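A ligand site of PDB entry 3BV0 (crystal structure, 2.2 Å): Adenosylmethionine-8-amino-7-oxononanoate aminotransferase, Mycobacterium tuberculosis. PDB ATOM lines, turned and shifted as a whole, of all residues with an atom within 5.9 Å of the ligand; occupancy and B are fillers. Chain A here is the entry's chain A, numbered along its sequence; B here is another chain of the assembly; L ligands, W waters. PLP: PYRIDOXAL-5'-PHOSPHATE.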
ATOM      1  N   TRP A  64      17.012 -18.471 -17.341  1.00  0.00           N
ATOM      2  CA  TRP A  64      17.018 -17.163 -17.974  1.00  0.00           C
ATOM      3  C   TRP A  64      18.154 -16.257 -17.505  1.00  0.00           C
ATOM      4  O   TRP A  64      17.910 -15.156 -16.975  1.00  0.00           O
ATOM      5  CB  TRP A  64      15.658 -16.465 -17.879  1.00  0.00           C
ATOM      6  CG  TRP A  64      15.393 -15.567 -19.069  1.00  0.00           C
ATOM      7  CD1 TRP A  64      15.643 -15.848 -20.386  1.00  0.00           C
ATOM      8  CD2 TRP A  64      14.817 -14.250 -19.051  1.00  0.00           C
ATOM      9  NE1 TRP A  64      15.274 -14.786 -21.187  1.00  0.00           N
ATOM     10  CE2 TRP A  64      14.761 -13.789 -20.388  1.00  0.00           C
ATOM     11  CE3 TRP A  64      14.354 -13.410 -18.034  1.00  0.00           C
ATOM     12  CZ2 TRP A  64      14.256 -12.534 -20.727  1.00  0.00           C
ATOM     13  CZ3 TRP A  64      13.848 -12.142 -18.384  1.00  0.00           C
ATOM     14  CH2 TRP A  64      13.797 -11.733 -19.721  1.00  0.00           C
ATOM     15  N   TRP A  65      19.374 -16.725 -17.772  1.00  0.00           N
ATOM     16  CA  TRP A  65      20.665 -16.064 -17.526  1.00  0.00           C
ATOM     17  C   TRP A  65      21.077 -15.976 -16.071  1.00  0.00           C
ATOM     18  O   TRP A  65      22.168 -15.498 -15.772  1.00  0.00           O
ATOM     19  CB  TRP A  65      20.728 -14.645 -18.122  1.00  0.00           C
ATOM     20  CG  TRP A  65      20.235 -14.424 -19.521  1.00  0.00           C
ATOM     21  CD1 TRP A  65      18.958 -14.188 -19.917  1.00  0.00           C
ATOM     22  CD2 TRP A  65      21.040 -14.336 -20.706  1.00  0.00           C
ATOM     23  NE1 TRP A  65      18.903 -13.982 -21.275  1.00  0.00           N
ATOM     24  CE2 TRP A  65      20.167 -14.068 -21.783  1.00  0.00           C
ATOM     25  CE3 TRP A  65      22.419 -14.476 -20.966  1.00  0.00           C
ATOM     26  CZ2 TRP A  65      20.614 -13.929 -23.108  1.00  0.00           C
ATOM     27  CZ3 TRP A  65      22.865 -14.341 -22.278  1.00  0.00           C
ATOM     28  CH2 TRP A  65      21.968 -14.071 -23.334  1.00  0.00           C
ATOM     29  N   ASP A 122      15.389  -3.357  -7.425  1.00  0.00           N
ATOM     30  CA  ASP A 122      14.857  -4.693  -7.252  1.00  0.00           C
ATOM     31  C   ASP A 122      14.658  -5.464  -8.562  1.00  0.00           C
ATOM     32  O   ASP A 122      14.375  -6.651  -8.528  1.00  0.00           O
ATOM     33  CB  ASP A 122      13.514  -4.620  -6.498  1.00  0.00           C
ATOM     34  CG  ASP A 122      13.655  -4.116  -5.071  1.00  0.00           C
ATOM     35  OD1 ASP A 122      14.704  -4.393  -4.429  1.00  0.00           O
ATOM     36  OD2 ASP A 122      12.721  -3.446  -4.586  1.00  0.00           O
ATOM     37  N   SER A 123      14.771  -4.795  -9.712  1.00  0.00           N
ATOM     38  CA  SER A 123      14.693  -5.482 -11.015  1.00  0.00           C
ATOM     39  C   SER A 123      15.440  -4.739 -12.139  1.00  0.00           C
ATOM     40  O   SER A 123      15.714  -3.545 -12.046  1.00  0.00           O
ATOM     41  CB  SER A 123      13.238  -5.677 -11.433  1.00  0.00           C
ATOM     42  OG  SER A 123      12.615  -4.420 -11.636  1.00  0.00           O
ATOM     43  N   GLY A 124      15.750  -5.480 -13.195  1.00  0.00           N
ATOM     44  CA  GLY A 124      16.441  -4.937 -14.374  1.00  0.00           C
ATOM     45  C   GLY A 124      15.677  -3.782 -14.989  1.00  0.00           C
ATOM     46  O   GLY A 124      16.240  -2.744 -15.280  1.00  0.00           O
ATOM     47  N   SER A 125      14.378  -3.972 -15.169  1.00  0.00           N
ATOM     48  CA  SER A 125      13.501  -2.909 -15.681  1.00  0.00           C
ATOM     49  C   SER A 125      13.558  -1.633 -14.871  1.00  0.00           C
ATOM     50  O   SER A 125      13.630  -0.542 -15.441  1.00  0.00           O
ATOM     51  CB  SER A 125      12.053  -3.386 -15.750  1.00  0.00           C
ATOM     52  OG  SER A 125      11.805  -4.031 -16.970  1.00  0.00           O
ATOM     53  N   VAL A 126      13.481  -1.751 -13.546  1.00  0.00           N
ATOM     54  CA  VAL A 126      13.576  -0.565 -12.692  1.00  0.00           C
ATOM     55  C   VAL A 126      14.957   0.070 -12.814  1.00  0.00           C
ATOM     56  O   VAL A 126      15.079   1.289 -12.840  1.00  0.00           O
ATOM     57  CB  VAL A 126      13.228  -0.863 -11.202  1.00  0.00           C
ATOM     58  CG1 VAL A 126      13.391   0.394 -10.313  1.00  0.00           C
ATOM     59  CG2 VAL A 126      11.809  -1.378 -11.079  1.00  0.00           C
ATOM     60  N   VAL A 128      16.836   0.144 -15.384  1.00  0.00           N
ATOM     61  CA  VAL A 128      16.821   0.836 -16.674  1.00  0.00           C
ATOM     62  C   VAL A 128      16.081   2.184 -16.568  1.00  0.00           C
ATOM     63  O   VAL A 128      16.488   3.198 -17.140  1.00  0.00           O
ATOM     64  CB  VAL A 128      16.173  -0.048 -17.751  1.00  0.00           C
ATOM     65  CG1 VAL A 128      15.865   0.767 -18.999  1.00  0.00           C
ATOM     66  CG2 VAL A 128      17.076  -1.250 -18.058  1.00  0.00           C
ATOM     67  N   TYR A 157      16.129  -5.236 -26.106  1.00  0.00           N
ATOM     68  CA  TYR A 157      15.182  -5.505 -25.046  1.00  0.00           C
ATOM     69  C   TYR A 157      15.741  -4.891 -23.774  1.00  0.00           C
ATOM     70  O   TYR A 157      16.902  -5.127 -23.426  1.00  0.00           O
ATOM     71  CB  TYR A 157      14.946  -7.013 -24.847  1.00  0.00           C
ATOM     72  CG  TYR A 157      14.033  -7.281 -23.658  1.00  0.00           C
ATOM     73  CD1 TYR A 157      12.695  -6.917 -23.706  1.00  0.00           C
ATOM     74  CD2 TYR A 157      14.523  -7.850 -22.476  1.00  0.00           C
ATOM     75  CE1 TYR A 157      11.862  -7.103 -22.633  1.00  0.00           C
ATOM     76  CE2 TYR A 157      13.674  -8.054 -21.380  1.00  0.00           C
ATOM     77  CZ  TYR A 157      12.348  -7.676 -21.475  1.00  0.00           C
ATOM     78  OH  TYR A 157      11.475  -7.872 -20.424  1.00  0.00           O
ATOM     79  N   HIS A 158      14.920  -4.113 -23.062  1.00  0.00           N
ATOM     80  CA  HIS A 158      15.379  -3.425 -21.838  1.00  0.00           C
ATOM     81  C   HIS A 158      14.467  -3.551 -20.637  1.00  0.00           C
ATOM     82  O   HIS A 158      14.661  -2.889 -19.618  1.00  0.00           O
ATOM     83  CB  HIS A 158      15.723  -1.962 -22.134  1.00  0.00           C
ATOM     84  CG  HIS A 158      16.739  -1.804 -23.219  1.00  0.00           C
ATOM     85  ND1 HIS A 158      18.081  -2.025 -23.004  1.00  0.00           N
ATOM     86  CD2 HIS A 158      16.596  -1.537 -24.531  1.00  0.00           C
ATOM     87  CE1 HIS A 158      18.725  -1.862 -24.147  1.00  0.00           C
ATOM     88  NE2 HIS A 158      17.853  -1.558 -25.088  1.00  0.00           N
ATOM     89  N   GLY A 159      13.484  -4.447 -20.733  1.00  0.00           N
ATOM     90  CA  GLY A 159      12.532  -4.612 -19.637  1.00  0.00           C
ATOM     91  C   GLY A 159      11.102  -4.347 -20.085  1.00  0.00           C
ATOM     92  O   GLY A 159      10.860  -3.999 -21.237  1.00  0.00           O
ATOM     93  N   ASP A 160      10.154  -4.486 -19.158  1.00  0.00           N
ATOM     94  CA  ASP A 160       8.748  -4.493 -19.518  1.00  0.00           C
ATOM     95  C   ASP A 160       7.934  -3.407 -18.821  1.00  0.00           C
ATOM     96  O   ASP A 160       6.726  -3.334 -18.976  1.00  0.00           O
ATOM     97  CB  ASP A 160       8.130  -5.873 -19.255  1.00  0.00           C
ATOM     98  CG  ASP A 160       7.138  -6.286 -20.330  1.00  0.00           C
ATOM     99  OD1 ASP A 160       6.494  -7.349 -20.173  1.00  0.00           O
ATOM    100  OD2 ASP A 160       6.986  -5.559 -21.344  1.00  0.00           O
ATOM    101  N   GLU A 220      22.302  -2.678 -25.622  1.00  0.00           N
ATOM    102  CA  GLU A 220      22.953  -3.881 -25.106  1.00  0.00           C
ATOM    103  C   GLU A 220      24.251  -4.054 -25.893  1.00  0.00           C
ATOM    104  O   GLU A 220      24.208  -4.110 -27.124  1.00  0.00           O
ATOM    105  CB  GLU A 220      22.082  -5.106 -25.327  1.00  0.00           C
ATOM    106  CG  GLU A 220      20.743  -5.092 -24.626  1.00  0.00           C
ATOM    107  CD  GLU A 220      19.749  -5.982 -25.326  1.00  0.00           C
ATOM    108  OE1 GLU A 220      19.082  -5.514 -26.288  1.00  0.00           O
ATOM    109  OE2 GLU A 220      19.628  -7.167 -24.928  1.00  0.00           O
ATOM    110  N   GLY A 225      19.992  -9.707 -26.208  1.00  0.00           N
ATOM    111  CA  GLY A 225      19.412 -10.941 -25.664  1.00  0.00           C
ATOM    112  C   GLY A 225      17.971 -11.254 -26.062  1.00  0.00           C
ATOM    113  O   GLY A 225      17.732 -11.917 -27.057  1.00  0.00           O
ATOM    114  N   ALA A 226      17.001 -10.782 -25.282  1.00  0.00           N
ATOM    115  CA  ALA A 226      15.600 -11.160 -25.503  1.00  0.00           C
ATOM    116  C   ALA A 226      15.044 -10.691 -26.845  1.00  0.00           C
ATOM    117  O   ALA A 226      13.994 -11.188 -27.285  1.00  0.00           O
ATOM    118  CB  ALA A 226      14.712 -10.674 -24.356  1.00  0.00           C
ATOM    119  N   ASP A 254      23.305  -1.352 -21.186  1.00  0.00           N
ATOM    120  CA  ASP A 254      22.469  -2.293 -20.482  1.00  0.00           C
ATOM    121  C   ASP A 254      23.134  -3.665 -20.492  1.00  0.00           C
ATOM    122  O   ASP A 254      23.028  -4.399 -21.478  1.00  0.00           O
ATOM    123  CB  ASP A 254      21.101  -2.366 -21.160  1.00  0.00           C
ATOM    124  CG  ASP A 254      20.137  -3.265 -20.434  1.00  0.00           C
ATOM    125  OD1 ASP A 254      20.589  -4.066 -19.603  1.00  0.00           O
ATOM    126  OD2 ASP A 254      18.916  -3.158 -20.677  1.00  0.00           O
ATOM    127  N   GLU A 255      23.838  -3.977 -19.401  1.00  0.00           N
ATOM    128  CA  GLU A 255      24.549  -5.259 -19.262  1.00  0.00           C
ATOM    129  C   GLU A 255      23.807  -6.254 -18.357  1.00  0.00           C
ATOM    130  O   GLU A 255      24.423  -7.108 -17.723  1.00  0.00           O
ATOM    131  CB  GLU A 255      25.973  -5.025 -18.733  1.00  0.00           C
ATOM    132  CG  GLU A 255      26.854  -4.148 -19.642  1.00  0.00           C
ATOM    133  CD  GLU A 255      28.127  -4.861 -20.061  1.00  0.00           C
ATOM    134  OE1 GLU A 255      28.167  -6.106 -19.951  1.00  0.00           O
ATOM    135  OE2 GLU A 255      29.077  -4.181 -20.488  1.00  0.00           O
ATOM    136  N   ILE A 256      22.487  -6.131 -18.280  1.00  0.00           N
ATOM    137  CA  ILE A 256      21.671  -6.970 -17.405  1.00  0.00           C
ATOM    138  C   ILE A 256      21.739  -8.472 -17.756  1.00  0.00           C
ATOM    139  O   ILE A 256      21.641  -9.334 -16.888  1.00  0.00           O
ATOM    140  CB  ILE A 256      20.213  -6.446 -17.324  1.00  0.00           C
ATOM    141  CG1 ILE A 256      20.167  -5.152 -16.505  1.00  0.00           C
ATOM    142  CG2 ILE A 256      19.282  -7.486 -16.717  1.00  0.00           C
ATOM    143  CD1 ILE A 256      18.920  -4.344 -16.692  1.00  0.00           C
ATOM    144  N   ALA A 257      21.915  -8.770 -19.041  1.00  0.00           N
ATOM    145  CA  ALA A 257      22.067 -10.146 -19.518  1.00  0.00           C
ATOM    146  C   ALA A 257      23.529 -10.492 -19.792  1.00  0.00           C
ATOM    147  O   ALA A 257      23.967 -11.632 -19.560  1.00  0.00           O
ATOM    148  CB  ALA A 257      21.237 -10.360 -20.757  1.00  0.00           C
ATOM    149  N   LYS A 283      20.167  -9.697 -13.316  1.00  0.00           N
ATOM    150  CA  LYS A 283      20.179 -11.154 -13.587  1.00  0.00           C
ATOM    151  C   LYS A 283      21.209 -12.004 -12.836  1.00  0.00           C
ATOM    152  O   LYS A 283      20.934 -12.508 -11.744  1.00  0.00           O
ATOM    153  CB  LYS A 283      20.175 -11.455 -15.091  1.00  0.00           C
ATOM    154  CG  LYS A 283      18.799 -11.285 -15.744  1.00  0.00           C
ATOM    155  CD  LYS A 283      18.889 -11.513 -17.247  1.00  0.00           C
ATOM    156  CE  LYS A 283      17.513 -11.482 -17.926  1.00  0.00           C
ATOM    157  NZ  LYS A 283      17.192 -10.144 -18.532  1.00  0.00           N
ATOM    158  N   ASP B 122       8.409  -8.028  -8.827  1.00  0.00           N
ATOM    159  CA  ASP B 122       9.492  -7.878  -7.861  1.00  0.00           C
ATOM    160  C   ASP B 122       9.393  -6.637  -6.981  1.00  0.00           C
ATOM    161  O   ASP B 122      10.089  -6.543  -5.967  1.00  0.00           O
ATOM    162  CB  ASP B 122      10.860  -7.863  -8.581  1.00  0.00           C
ATOM    163  CG  ASP B 122      11.122  -9.152  -9.369  1.00  0.00           C
ATOM    164  OD1 ASP B 122      10.956 -10.245  -8.787  1.00  0.00           O
ATOM    165  OD2 ASP B 122      11.506  -9.057 -10.558  1.00  0.00           O
ATOM    166  N   GLY B 316       6.924 -10.791 -18.489  1.00  0.00           N
ATOM    167  CA  GLY B 316       7.215 -11.033 -17.058  1.00  0.00           C
ATOM    168  C   GLY B 316       8.613 -10.637 -16.596  1.00  0.00           C
ATOM    169  O   GLY B 316       9.572 -10.682 -17.382  1.00  0.00           O
ATOM    170  N   PRO B 317       8.746 -10.238 -15.325  1.00  0.00           N
ATOM    171  CA  PRO B 317      10.079 -10.003 -14.760  1.00  0.00           C
ATOM    172  C   PRO B 317      10.919 -11.287 -14.676  1.00  0.00           C
ATOM    173  O   PRO B 317      10.376 -12.365 -14.460  1.00  0.00           O
ATOM    174  CB  PRO B 317       9.797  -9.461 -13.343  1.00  0.00           C
ATOM    175  CG  PRO B 317       8.340  -9.364 -13.184  1.00  0.00           C
ATOM    176  CD  PRO B 317       7.648  -9.963 -14.370  1.00  0.00           C
ATOM    177  N   THR B 318      12.230 -11.148 -14.842  1.00  0.00           N
ATOM    178  CA  THR B 318      13.185 -12.250 -14.650  1.00  0.00           C
ATOM    179  C   THR B 318      12.947 -13.115 -13.405  1.00  0.00           C
ATOM    180  O   THR B 318      12.961 -14.341 -13.492  1.00  0.00           O
ATOM    181  CB  THR B 318      14.628 -11.712 -14.579  1.00  0.00           C
ATOM    182  OG1 THR B 318      14.883 -10.919 -15.746  1.00  0.00           O
ATOM    183  CG2 THR B 318      15.640 -12.866 -14.521  1.00  0.00           C
ATOM    184  N   PHE B 319      12.741 -12.494 -12.246  1.00  0.00           N
ATOM    185  CA  PHE B 319      12.538 -13.262 -11.000  1.00  0.00           C
ATOM    186  C   PHE B 319      11.081 -13.425 -10.612  1.00  0.00           C
ATOM    187  O   PHE B 319      10.765 -13.691  -9.457  1.00  0.00           O
ATOM    188  CB  PHE B 319      13.341 -12.664  -9.840  1.00  0.00           C
ATOM    189  CG  PHE B 319      14.804 -12.881  -9.974  1.00  0.00           C
ATOM    190  CD1 PHE B 319      15.394 -14.008  -9.420  1.00  0.00           C
ATOM    191  CD2 PHE B 319      15.592 -11.978 -10.671  1.00  0.00           C
ATOM    192  CE1 PHE B 319      16.753 -14.231  -9.573  1.00  0.00           C
ATOM    193  CE2 PHE B 319      16.949 -12.183 -10.819  1.00  0.00           C
ATOM    194  CZ  PHE B 319      17.526 -13.320 -10.270  1.00  0.00           C
HETATM  195  N1  PLP L   1      17.554  -5.436 -19.910  1.00  0.00           N
HETATM  196  C2  PLP L   1      18.102  -6.586 -20.438  1.00  0.00           C
HETATM  197  C2A PLP L   1      19.227  -6.527 -21.421  1.00  0.00           C
HETATM  198  C3  PLP L   1      17.591  -7.814 -20.040  1.00  0.00           C
HETATM  199  O3  PLP L   1      18.119  -8.965 -20.577  1.00  0.00           O
HETATM  200  C4  PLP L   1      16.550  -7.883 -19.103  1.00  0.00           C
HETATM  201  C4A PLP L   1      16.425  -9.161 -18.325  1.00  0.00           C
HETATM  202  C5  PLP L   1      16.008  -6.711 -18.576  1.00  0.00           C
HETATM  203  C6  PLP L   1      16.529  -5.486 -18.995  1.00  0.00           C
HETATM  204  C5A PLP L   1      14.849  -6.711 -17.594  1.00  0.00           C
HETATM  205  O4P PLP L   1      15.152  -7.223 -16.312  1.00  0.00           O
HETATM  206  P   PLP L   1      13.958  -7.698 -15.321  1.00  0.00           P
HETATM  207  O1P PLP L   1      13.291  -8.880 -16.004  1.00  0.00           O
HETATM  208  O2P PLP L   1      12.955  -6.607 -15.070  1.00  0.00           O
HETATM  209  O3P PLP L   1      14.509  -8.129 -13.969  1.00  0.00           O
HETATM  210  O   HOH W   1      10.591  -5.814 -13.397  1.00  0.00           O
HETATM  211  O   HOH W   2      17.308  -8.721 -12.942  1.00  0.00           O
HETATM  212  O   HOH W   3      17.949  -9.071 -23.401  1.00  0.00           O
HETATM  213  O   HOH W   4      10.191  -6.599 -17.042  1.00  0.00           O
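A carbon (C4A) of the ligand is bonded to the side-chain amino group (NZ) of Lys 283 (1.3 Å). N of Thr 318 of chain B lies within hydrogen-bond range of O1P of the ligand, 2.8 Å away. OG1 of Thr 318 of chain B is in hydrogen-bond range of O1P of the ligand. The side-chain carboxylate of Asp 254 sits at hydrogen-bond distance from a nitrogen (N1) of the ligand (2.8 Å). The backbone NH of Ser 125 is in hydrogen-bond range of an oxygen (O2P) of the ligand (3.0 Å). An oxygen (O2P) of the ligand sits at hydrogen-bond distance from the side-chain hydroxyl (OG) of Ser 125. N of Gly 124 is in hydrogen-bond range of O3P of the ligand.
Residues that only touch the ligand: His 158 (3.3 Å), Tyr 157 (3.4 Å), Ala 257 (3.4 Å), Ile 256 (3.5 Å), Glu 220 (3.6 Å), Pro 317 of chain B (3.6 Å), Gly 159 (3.7 Å), Ser 123 (3.7 Å) and Trp 64 (3.9 Å). The nearest printed residue that does not touch the ligand is Gly 316 of chain B (4.4 Å).
OD2 of Asp 254 is in hydrogen-bond range of ND1 of His 158, 2.7 Å away. OD1 of Asp 254 sits at hydrogen-bond distance from N of Ile 256, at 3.1 Å. N of Asp 160 is in hydrogen-bond range of OG of Ser 125. The backbone NH of Tyr 157 lies within hydrogen-bond range of the side-chain carboxylate of Glu 220 (3.0 Å). OE2 of Glu 220 is in hydrogen-bond range of N of Gly 225 (2.9 Å). The side-chain hydroxyl of Ser 123 sits close to the backbone NH of Val 126.
Water W3 lies within hydrogen-bond range of N of Ala 226 (2.7 Å), O3 of the ligand (2.8 Å) and OE2 of Glu 220 (3.0 Å). Water W1 bridges O2P of the ligand and OG of Ser 123. Water W2 lies within hydrogen-bond range of O3P of the ligand and N of Lys 283. Water W4 lies within hydrogen-bond range of the backbone NH of Asp 160 (3.0 Å), the side-chain hydroxyl of Ser 125 (3.0 Å) and an oxygen (O2P) of the ligand (3.4 Å).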
